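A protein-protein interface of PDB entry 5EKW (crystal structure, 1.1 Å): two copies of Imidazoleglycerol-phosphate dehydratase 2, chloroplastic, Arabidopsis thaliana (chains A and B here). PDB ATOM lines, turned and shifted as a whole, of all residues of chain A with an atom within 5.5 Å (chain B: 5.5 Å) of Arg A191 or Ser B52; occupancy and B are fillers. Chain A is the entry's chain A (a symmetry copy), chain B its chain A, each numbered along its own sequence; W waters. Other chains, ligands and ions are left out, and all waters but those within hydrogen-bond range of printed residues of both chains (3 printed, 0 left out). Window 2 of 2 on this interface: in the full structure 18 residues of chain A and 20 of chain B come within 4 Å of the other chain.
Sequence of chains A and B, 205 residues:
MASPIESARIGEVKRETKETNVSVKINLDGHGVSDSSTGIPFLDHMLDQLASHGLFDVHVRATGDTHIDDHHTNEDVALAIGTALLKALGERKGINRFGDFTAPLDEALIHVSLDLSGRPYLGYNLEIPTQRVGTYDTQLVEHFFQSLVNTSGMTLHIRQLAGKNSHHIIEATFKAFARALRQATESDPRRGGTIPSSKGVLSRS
O of Gly A94 sits at hydrogen-bond distance from N of Asp A188 (2.8 Å).
The guanidinium group of Arg B179 sits at hydrogen-bond distance from a ring nitrogen (ND1) of His B53 (3.0 Å).
OD1 of Asp A188 is in hydrogen-bond range of N of Arg A190 (2.9 Å).
The side-chain hydroxyl (OG) of Ser B52 sits at hydrogen-bond distance from the backbone carbonyl oxygen (O) of Asp B48.
N of Gly B32 is in hydrogen-bond range of O of Leu B55 (3.2 Å).
The backbone carbonyl oxygen (O) of Arg A191 is in hydrogen-bond range of the side-chain hydroxyl (OG1) of Thr A194 (2.7 Å).
Among the printed residues, pairs that only touch across the chains: Arg A190 with Leu B55 (3.3 Å), Pro A196 with His B53 (3.4 Å), Ser A198 with Ser B52 (3.7 Å) and Arg A190 with Arg B182 (3.8 Å).
Water W1 bridges the backbone carbonyl oxygen of Gly B54 (2.7 Å) and the guanidinium group of Arg A190 (2.8 Å).
Water W2 lies within hydrogen-bond range of the side-chain amide oxygen of Gln B49 (2.8 Å), a ring nitrogen (NE2) of His B53 (2.8 Å) and the backbone NH of Ser A198 (2.9 Å).
Water W3 lies within hydrogen-bond range of OD2 of Asp A188 (2.8 Å), NH2 of Arg A191 (2.9 Å), O of Ile A95 (3.0 Å) and NH1 of Arg B179 (3.1 Å).
Printed residues of chain B within 4 Å of Asp A188: Arg B182 (2.8 Å).
Of the printed residues of chain B, Arg A191 touches Ser B52 (3.1 Å).
Of the printed residues of chain B, Ser A198 touches Gln B49 (2.9 Å) and Ser B52 (3.7 Å).
Of the printed residues of chain A, Gln B49 touches Ser A198 (2.9 Å).
Ser B52 touches just these residues of chain A: Arg A191 (3.1 Å) and Ser A198 (3.7 Å).
Of the printed residues of chain A, His B53 touches Pro A196 (3.4 Å).
Of the printed residues of chain A, Arg B182 touches Asp A188 (2.8 Å) and Arg A190 (3.8 Å).
The nearest printed residue of chain A that does not touch His B53 is Ser A197 (4.4 Å).
NE2 of Gln B49 sits at hydrogen-bond distance from OG of Ser A198 (2.9 Å).
O of Ser B52 sits at hydrogen-bond distance from NH2 of Arg A191, 3.1 Å away.
NH2 of Arg B182 lies within salt-bridge range of OD1 of Asp A188.
No position is printed for both chains.
Of the 7 pairs that touch across the chains among the printed residues, none has its exchanged pair printed and touching as well.
Of the 13 printed residues of chain A, 5 touch a printed residue of chain B.
Printed residues of chain A that touch a printed residue of chain B: Asp A188, Arg A190, Arg A191, Pro A196 and Ser A198.
Printed residues of chain B that touch a printed residue of chain A: Gln B49, Ser B52, His B53, Leu B55 and Arg B182.
Among the printed residues, 7 pairs touch across the chains.
Among the printed residues, Asp or Glu carboxylates within 4 Å of a Lys or Arg side-chain nitrogen of the other chain: Asp A188 with Arg B182 (2.8 Å).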
ATOM      1  N   GLY A  94      17.561  30.991  24.757  1.00  0.00           N
ATOM      2  CA  GLY A  94      16.961  31.476  23.505  1.00  0.00           C
ATOM      3  C   GLY A  94      17.400  32.836  22.987  1.00  0.00           C
ATOM      4  O   GLY A  94      16.821  33.322  22.031  1.00  0.00           O
ATOM      5  N   ILE A  95      18.410  33.435  23.612  1.00  0.00           N
ATOM      6  CA  ILE A  95      18.845  34.801  23.270  1.00  0.00           C
ATOM      7  C   ILE A  95      19.936  34.800  22.214  1.00  0.00           C
ATOM      8  O   ILE A  95      20.633  33.816  22.015  1.00  0.00           O
ATOM      9  CB  ILE A  95      19.276  35.633  24.504  1.00  0.00           C
ATOM     10  CG1 ILE A  95      20.575  35.124  25.124  1.00  0.00           C
ATOM     11  CG2 ILE A  95      18.120  35.704  25.488  1.00  0.00           C
ATOM     12  CD1 ILE A  95      21.135  36.040  26.198  1.00  0.00           C
ATOM     13  N   ASP A 188      16.703  34.963  19.743  1.00  0.00           N
ATOM     14  CA  ASP A 188      17.222  34.381  18.509  1.00  0.00           C
ATOM     15  C   ASP A 188      16.072  33.561  17.919  1.00  0.00           C
ATOM     16  O   ASP A 188      15.682  32.570  18.514  1.00  0.00           O
ATOM     17  CB  ASP A 188      18.455  33.517  18.805  1.00  0.00           C
ATOM     18  CG  ASP A 188      19.048  32.880  17.568  1.00  0.00           C
ATOM     19  OD1 ASP A 188      18.299  32.606  16.601  1.00  0.00           O
ATOM     20  OD2 ASP A 188      20.274  32.620  17.569  1.00  0.00           O
ATOM     21  N   PRO A 189      15.541  33.949  16.738  1.00  0.00           N
ATOM     22  CA  PRO A 189      14.342  33.274  16.230  1.00  0.00           C
ATOM     23  C   PRO A 189      14.532  31.832  15.804  1.00  0.00           C
ATOM     24  O   PRO A 189      13.543  31.121  15.592  1.00  0.00           O
ATOM     25  CB  PRO A 189      13.964  34.116  15.016  1.00  0.00           C
ATOM     26  CG  PRO A 189      15.244  34.705  14.550  1.00  0.00           C
ATOM     27  CD  PRO A 189      16.006  34.988  15.811  1.00  0.00           C
ATOM     28  N   ARG A 190      15.777  31.408  15.664  1.00  0.00           N
ATOM     29  CA  ARG A 190      16.047  30.039  15.243  1.00  0.00           C
ATOM     30  C   ARG A 190      16.452  29.058  16.306  1.00  0.00           C
ATOM     31  O   ARG A 190      16.459  27.864  16.041  1.00  0.00           O
ATOM     32  CB  ARG A 190      17.115  30.004  14.166  1.00  0.00           C
ATOM     33  CG  ARG A 190      16.628  30.514  12.830  1.00  0.00           C
ATOM     34  CD  ARG A 190      17.728  30.493  11.787  1.00  0.00           C
ATOM     35  NE  ARG A 190      18.248  29.149  11.517  1.00  0.00           N
ATOM     36  CZ  ARG A 190      19.368  28.910  10.840  1.00  0.00           C
ATOM     37  NH1 ARG A 190      20.087  29.921  10.362  1.00  0.00           N
ATOM     38  NH2 ARG A 190      19.773  27.655  10.640  1.00  0.00           N
ATOM     39  N   ARG A 191      16.838  29.509  17.481  1.00  0.00           N
ATOM     40  CA  ARG A 191      17.521  28.544  18.343  1.00  0.00           C
ATOM     41  C   ARG A 191      16.629  27.815  19.350  1.00  0.00           C
ATOM     42  O   ARG A 191      17.121  27.014  20.149  1.00  0.00           O
ATOM     43  CB  ARG A 191      18.746  29.153  18.961  1.00  0.00           C
ATOM     44  CG  ARG A 191      18.534  29.905  20.236  1.00  0.00           C
ATOM     45  CD  ARG A 191      19.915  30.267  20.788  1.00  0.00           C
ATOM     46  NE  ARG A 191      20.775  29.063  20.802  1.00  0.00           N
ATOM     47  CZ  ARG A 191      21.923  28.840  20.125  1.00  0.00           C
ATOM     48  NH1 ARG A 191      22.498  27.653  20.226  1.00  0.00           N
ATOM     49  NH2 ARG A 191      22.531  29.756  19.378  1.00  0.00           N
ATOM     50  N   GLY A 192      15.334  28.114  19.290  1.00  0.00           N
ATOM     51  CA  GLY A 192      14.282  27.314  19.950  1.00  0.00           C
ATOM     52  C   GLY A 192      14.427  27.147  21.453  1.00  0.00           C
ATOM     53  O   GLY A 192      14.260  26.057  21.995  1.00  0.00           O
ATOM     54  N   GLY A 193      14.760  28.242  22.115  1.00  0.00           N
ATOM     55  CA  GLY A 193      14.909  28.286  23.588  1.00  0.00           C
ATOM     56  C   GLY A 193      16.106  27.572  24.207  1.00  0.00           C
ATOM     57  O   GLY A 193      16.167  27.404  25.422  1.00  0.00           O
ATOM     58  N   THR A 194      17.037  27.128  23.373  1.00  0.00           N
ATOM     59  CA  THR A 194      18.289  26.513  23.859  1.00  0.00           C
ATOM     60  C   THR A 194      19.245  27.589  24.408  1.00  0.00           C
ATOM     61  O   THR A 194      19.171  28.752  24.011  1.00  0.00           O
ATOM     62  CB  THR A 194      19.001  25.666  22.771  1.00  0.00           C
ATOM     63  OG1 THR A 194      19.361  26.489  21.650  1.00  0.00           O
ATOM     64  CG2 THR A 194      18.098  24.514  22.312  1.00  0.00           C
ATOM     65  N   ILE A 195      20.124  27.192  25.327  1.00  0.00           N
ATOM     66  CA  ILE A 195      21.174  28.101  25.842  1.00  0.00           C
ATOM     67  C   ILE A 195      22.215  28.264  24.723  1.00  0.00           C
ATOM     68  O   ILE A 195      22.677  27.262  24.169  1.00  0.00           O
ATOM     69  CB  ILE A 195      21.837  27.595  27.145  1.00  0.00           C
ATOM     70  CG1 ILE A 195      20.809  27.629  28.288  1.00  0.00           C
ATOM     71  CG2 ILE A 195      23.053  28.456  27.505  1.00  0.00           C
ATOM     72  CD1 ILE A 195      21.198  26.821  29.506  1.00  0.00           C
ATOM     73  N   PRO A 196      22.584  29.511  24.376  1.00  0.00           N
ATOM     74  CA  PRO A 196      23.504  29.726  23.246  1.00  0.00           C
ATOM     75  C   PRO A 196      24.968  29.543  23.639  1.00  0.00           C
ATOM     76  O   PRO A 196      25.732  30.497  23.756  1.00  0.00           O
ATOM     77  CB  PRO A 196      23.190  31.145  22.815  1.00  0.00           C
ATOM     78  CG  PRO A 196      22.797  31.800  24.080  1.00  0.00           C
ATOM     79  CD  PRO A 196      22.014  30.776  24.850  1.00  0.00           C
ATOM     80  N   SER A 197      25.337  28.296  23.835  1.00  0.00           N
ATOM     81  CA  SER A 197      26.679  27.914  24.259  1.00  0.00           C
ATOM     82  C   SER A 197      26.900  26.451  23.908  1.00  0.00           C
ATOM     83  O   SER A 197      25.968  25.657  23.946  1.00  0.00           O
ATOM     84  CB  SER A 197      26.870  28.114  25.771  1.00  0.00           C
ATOM     85  OG  SER A 197      28.142  27.645  26.193  1.00  0.00           O
ATOM     86  N   SER A 198      28.134  26.113  23.565  1.00  0.00           N
ATOM     87  CA  SER A 198      28.520  24.713  23.364  1.00  0.00           C
ATOM     88  C   SER A 198      28.771  23.948  24.668  1.00  0.00           C
ATOM     89  O   SER A 198      28.853  22.725  24.642  1.00  0.00           O
ATOM     90  CB  SER A 198      29.782  24.631  22.511  1.00  0.00           C
ATOM     91  OG  SER A 198      30.851  25.329  23.141  1.00  0.00           O
ATOM     92  N   GLY B  32      21.925  23.620  14.690  1.00  0.00           N
ATOM     93  CA  GLY B  32      23.157  23.605  15.479  1.00  0.00           C
ATOM     94  C   GLY B  32      23.616  22.242  15.957  1.00  0.00           C
ATOM     95  O   GLY B  32      24.292  22.142  16.981  1.00  0.00           O
ATOM     96  N   LEU B  47      34.830  23.515  15.362  1.00  0.00           N
ATOM     97  CA  LEU B  47      33.679  23.140  14.516  1.00  0.00           C
ATOM     98  C   LEU B  47      32.376  23.083  15.309  1.00  0.00           C
ATOM     99  O   LEU B  47      31.301  23.337  14.770  1.00  0.00           O
ATOM    100  CB  LEU B  47      33.961  21.828  13.790  1.00  0.00           C
ATOM    101  CG  LEU B  47      35.073  21.908  12.735  1.00  0.00           C
ATOM    102  CD1 LEU B  47      35.409  20.533  12.189  1.00  0.00           C
ATOM    103  CD2 LEU B  47      34.703  22.840  11.594  1.00  0.00           C
ATOM    104  N   ASP B  48      32.475  22.755  16.589  1.00  0.00           N
ATOM    105  CA  ASP B  48      31.308  22.879  17.478  1.00  0.00           C
ATOM    106  C   ASP B  48      30.791  24.307  17.632  1.00  0.00           C
ATOM    107  O   ASP B  48      29.586  24.493  17.762  1.00  0.00           O
ATOM    108  CB  ASP B  48      31.613  22.313  18.847  1.00  0.00           C
ATOM    109  CG  ASP B  48      31.766  20.823  18.835  1.00  0.00           C
ATOM    110  OD1 ASP B  48      31.397  20.155  17.830  1.00  0.00           O
ATOM    111  OD2 ASP B  48      32.206  20.277  19.862  1.00  0.00           O
ATOM    112  N   GLN B  49      31.681  25.302  17.619  1.00  0.00           N
ATOM    113  CA  GLN B  49      31.211  26.714  17.663  1.00  0.00           C
ATOM    114  C   GLN B  49      30.498  27.060  16.389  1.00  0.00           C
ATOM    115  O   GLN B  49      29.561  27.843  16.379  1.00  0.00           O
ATOM    116  CB  GLN B  49      32.345  27.713  17.874  1.00  0.00           C
ATOM    117  CG  GLN B  49      33.203  27.396  19.073  1.00  0.00           C
ATOM    118  CD  GLN B  49      32.392  27.144  20.316  1.00  0.00           C
ATOM    119  OE1 GLN B  49      31.530  27.949  20.690  1.00  0.00           O
ATOM    120  NE2 GLN B  49      32.627  26.010  20.939  1.00  0.00           N
ATOM    121  N   LEU B  50      31.037  26.530  15.290  1.00  0.00           N
ATOM    122  CA  LEU B  50      30.444  26.766  13.981  1.00  0.00           C
ATOM    123  C   LEU B  50      28.976  26.307  14.021  1.00  0.00           C
ATOM    124  O   LEU B  50      28.072  27.007  13.585  1.00  0.00           O
ATOM    125  CB  LEU B  50      31.247  26.061  12.887  1.00  0.00           C
ATOM    126  CG  LEU B  50      30.681  26.204  11.475  1.00  0.00           C
ATOM    127  CD1 LEU B  50      30.566  27.654  11.035  1.00  0.00           C
ATOM    128  CD2 LEU B  50      31.542  25.407  10.513  1.00  0.00           C
ATOM    129  N   ALA B  51      28.755  25.121  14.581  1.00  0.00           N
ATOM    130  CA  ALA B  51      27.397  24.604  14.731  1.00  0.00           C
ATOM    131  C   ALA B  51      26.561  25.397  15.754  1.00  0.00           C
ATOM    132  O   ALA B  51      25.451  25.844  15.454  1.00  0.00           O
ATOM    133  CB  ALA B  51      27.439  23.130  15.091  1.00  0.00           C
ATOM    134  N   SER B  52      27.115  25.576  16.951  1.00  0.00           N
ATOM    135  CA  SER B  52      26.358  26.218  18.057  1.00  0.00           C
ATOM    136  C   SER B  52      25.983  27.667  17.776  1.00  0.00           C
ATOM    137  O   SER B  52      24.907  28.110  18.183  1.00  0.00           O
ATOM    138  CB  SER B  52      27.112  26.204  19.394  1.00  0.00           C
ATOM    139  OG  SER B  52      27.188  24.925  19.960  1.00  0.00           O
ATOM    140  N   HIS B  53      26.895  28.407  17.140  1.00  0.00           N
ATOM    141  CA  HIS B  53      26.677  29.858  16.895  1.00  0.00           C
ATOM    142  C   HIS B  53      26.193  30.193  15.509  1.00  0.00           C
ATOM    143  O   HIS B  53      25.548  31.199  15.305  1.00  0.00           O
ATOM    144  CB  HIS B  53      27.877  30.656  17.324  1.00  0.00           C
ATOM    145  CG  HIS B  53      28.063  30.563  18.794  1.00  0.00           C
ATOM    146  ND1 HIS B  53      27.150  31.092  19.687  1.00  0.00           N
ATOM    147  CD2 HIS B  53      28.922  29.819  19.524  1.00  0.00           C
ATOM    148  CE1 HIS B  53      27.500  30.759  20.912  1.00  0.00           C
ATOM    149  NE2 HIS B  53      28.579  29.995  20.842  1.00  0.00           N
ATOM    150  N   GLY B  54      26.485  29.316  14.566  1.00  0.00           N
ATOM    151  CA  GLY B  54      25.983  29.483  13.196  1.00  0.00           C
ATOM    152  C   GLY B  54      24.651  28.797  12.943  1.00  0.00           C
ATOM    153  O   GLY B  54      23.997  29.101  11.963  1.00  0.00           O
ATOM    154  N   LEU B  55      24.270  27.883  13.840  1.00  0.00           N
ATOM    155  CA  LEU B  55      23.088  27.004  13.687  1.00  0.00           C
ATOM    156  C   LEU B  55      23.156  26.086  12.475  1.00  0.00           C
ATOM    157  O   LEU B  55      22.171  25.495  12.074  1.00  0.00           O
ATOM    158  CB  LEU B  55      21.767  27.785  13.751  1.00  0.00           C
ATOM    159  CG  LEU B  55      21.536  28.407  15.137  1.00  0.00           C
ATOM    160  CD1 LEU B  55      20.198  29.108  15.111  1.00  0.00           C
ATOM    161  CD2 LEU B  55      21.620  27.397  16.277  1.00  0.00           C
ATOM    162  N   PHE B  56      24.342  25.899  11.933  1.00  0.00           N
ATOM    163  CA  PHE B  56      24.569  24.847  10.948  1.00  0.00           C
ATOM    164  C   PHE B  56      24.504  23.496  11.625  1.00  0.00           C
ATOM    165  O   PHE B  56      24.888  23.376  12.779  1.00  0.00           O
ATOM    166  CB  PHE B  56      25.934  25.044  10.299  1.00  0.00           C
ATOM    167  CG  PHE B  56      26.076  26.393   9.663  1.00  0.00           C
ATOM    168  CD1 PHE B  56      25.380  26.674   8.505  1.00  0.00           C
ATOM    169  CD2 PHE B  56      26.819  27.411  10.251  1.00  0.00           C
ATOM    170  CE1 PHE B  56      25.429  27.925   7.913  1.00  0.00           C
ATOM    171  CE2 PHE B  56      26.883  28.661   9.653  1.00  0.00           C
ATOM    172  CZ  PHE B  56      26.182  28.922   8.498  1.00  0.00           C
ATOM    173  N   ARG B 179      28.747  33.344  12.888  1.00  0.00           N
ATOM    174  CA  ARG B 179      27.649  34.317  12.868  1.00  0.00           C
ATOM    175  C   ARG B 179      27.597  35.058  11.542  1.00  0.00           C
ATOM    176  O   ARG B 179      26.510  35.315  11.008  1.00  0.00           O
ATOM    177  CB  ARG B 179      27.731  35.249  14.088  1.00  0.00           C
ATOM    178  CG  ARG B 179      27.396  34.463  15.368  1.00  0.00           C
ATOM    179  CD  ARG B 179      27.355  35.106  16.744  1.00  0.00           C
ATOM    180  NE  ARG B 179      26.733  34.124  17.682  1.00  0.00           N
ATOM    181  CZ  ARG B 179      25.447  34.075  18.085  1.00  0.00           C
ATOM    182  NH1 ARG B 179      25.035  33.078  18.877  1.00  0.00           N
ATOM    183  NH2 ARG B 179      24.545  34.991  17.733  1.00  0.00           N
ATOM    184  N   ARG B 182      26.256  32.468   8.988  1.00  0.00           N
ATOM    185  CA  ARG B 182      24.813  32.335   9.226  1.00  0.00           C
ATOM    186  C   ARG B 182      24.065  33.501   8.542  1.00  0.00           C
ATOM    187  O   ARG B 182      23.126  33.276   7.783  1.00  0.00           O
ATOM    188  CB  ARG B 182      24.535  32.275  10.723  1.00  0.00           C
ATOM    189  CG  ARG B 182      23.054  32.346  11.037  1.00  0.00           C
ATOM    190  CD  ARG B 182      22.803  32.291  12.520  1.00  0.00           C
ATOM    191  NE  ARG B 182      21.407  32.565  12.799  1.00  0.00           N
ATOM    192  CZ  ARG B 182      20.858  32.547  14.005  1.00  0.00           C
ATOM    193  NH1 ARG B 182      21.581  32.237  15.064  1.00  0.00           N
ATOM    194  NH2 ARG B 182      19.570  32.845  14.126  1.00  0.00           N
HETATM  195  O   HOH W   1      22.496  28.532   9.764  1.00  0.00           O
HETATM  196  O   HOH W   2      29.791  28.395  22.813  1.00  0.00           O
HETATM  197  O   HOH W   3      22.082  32.622  19.697  1.00  0.00           O
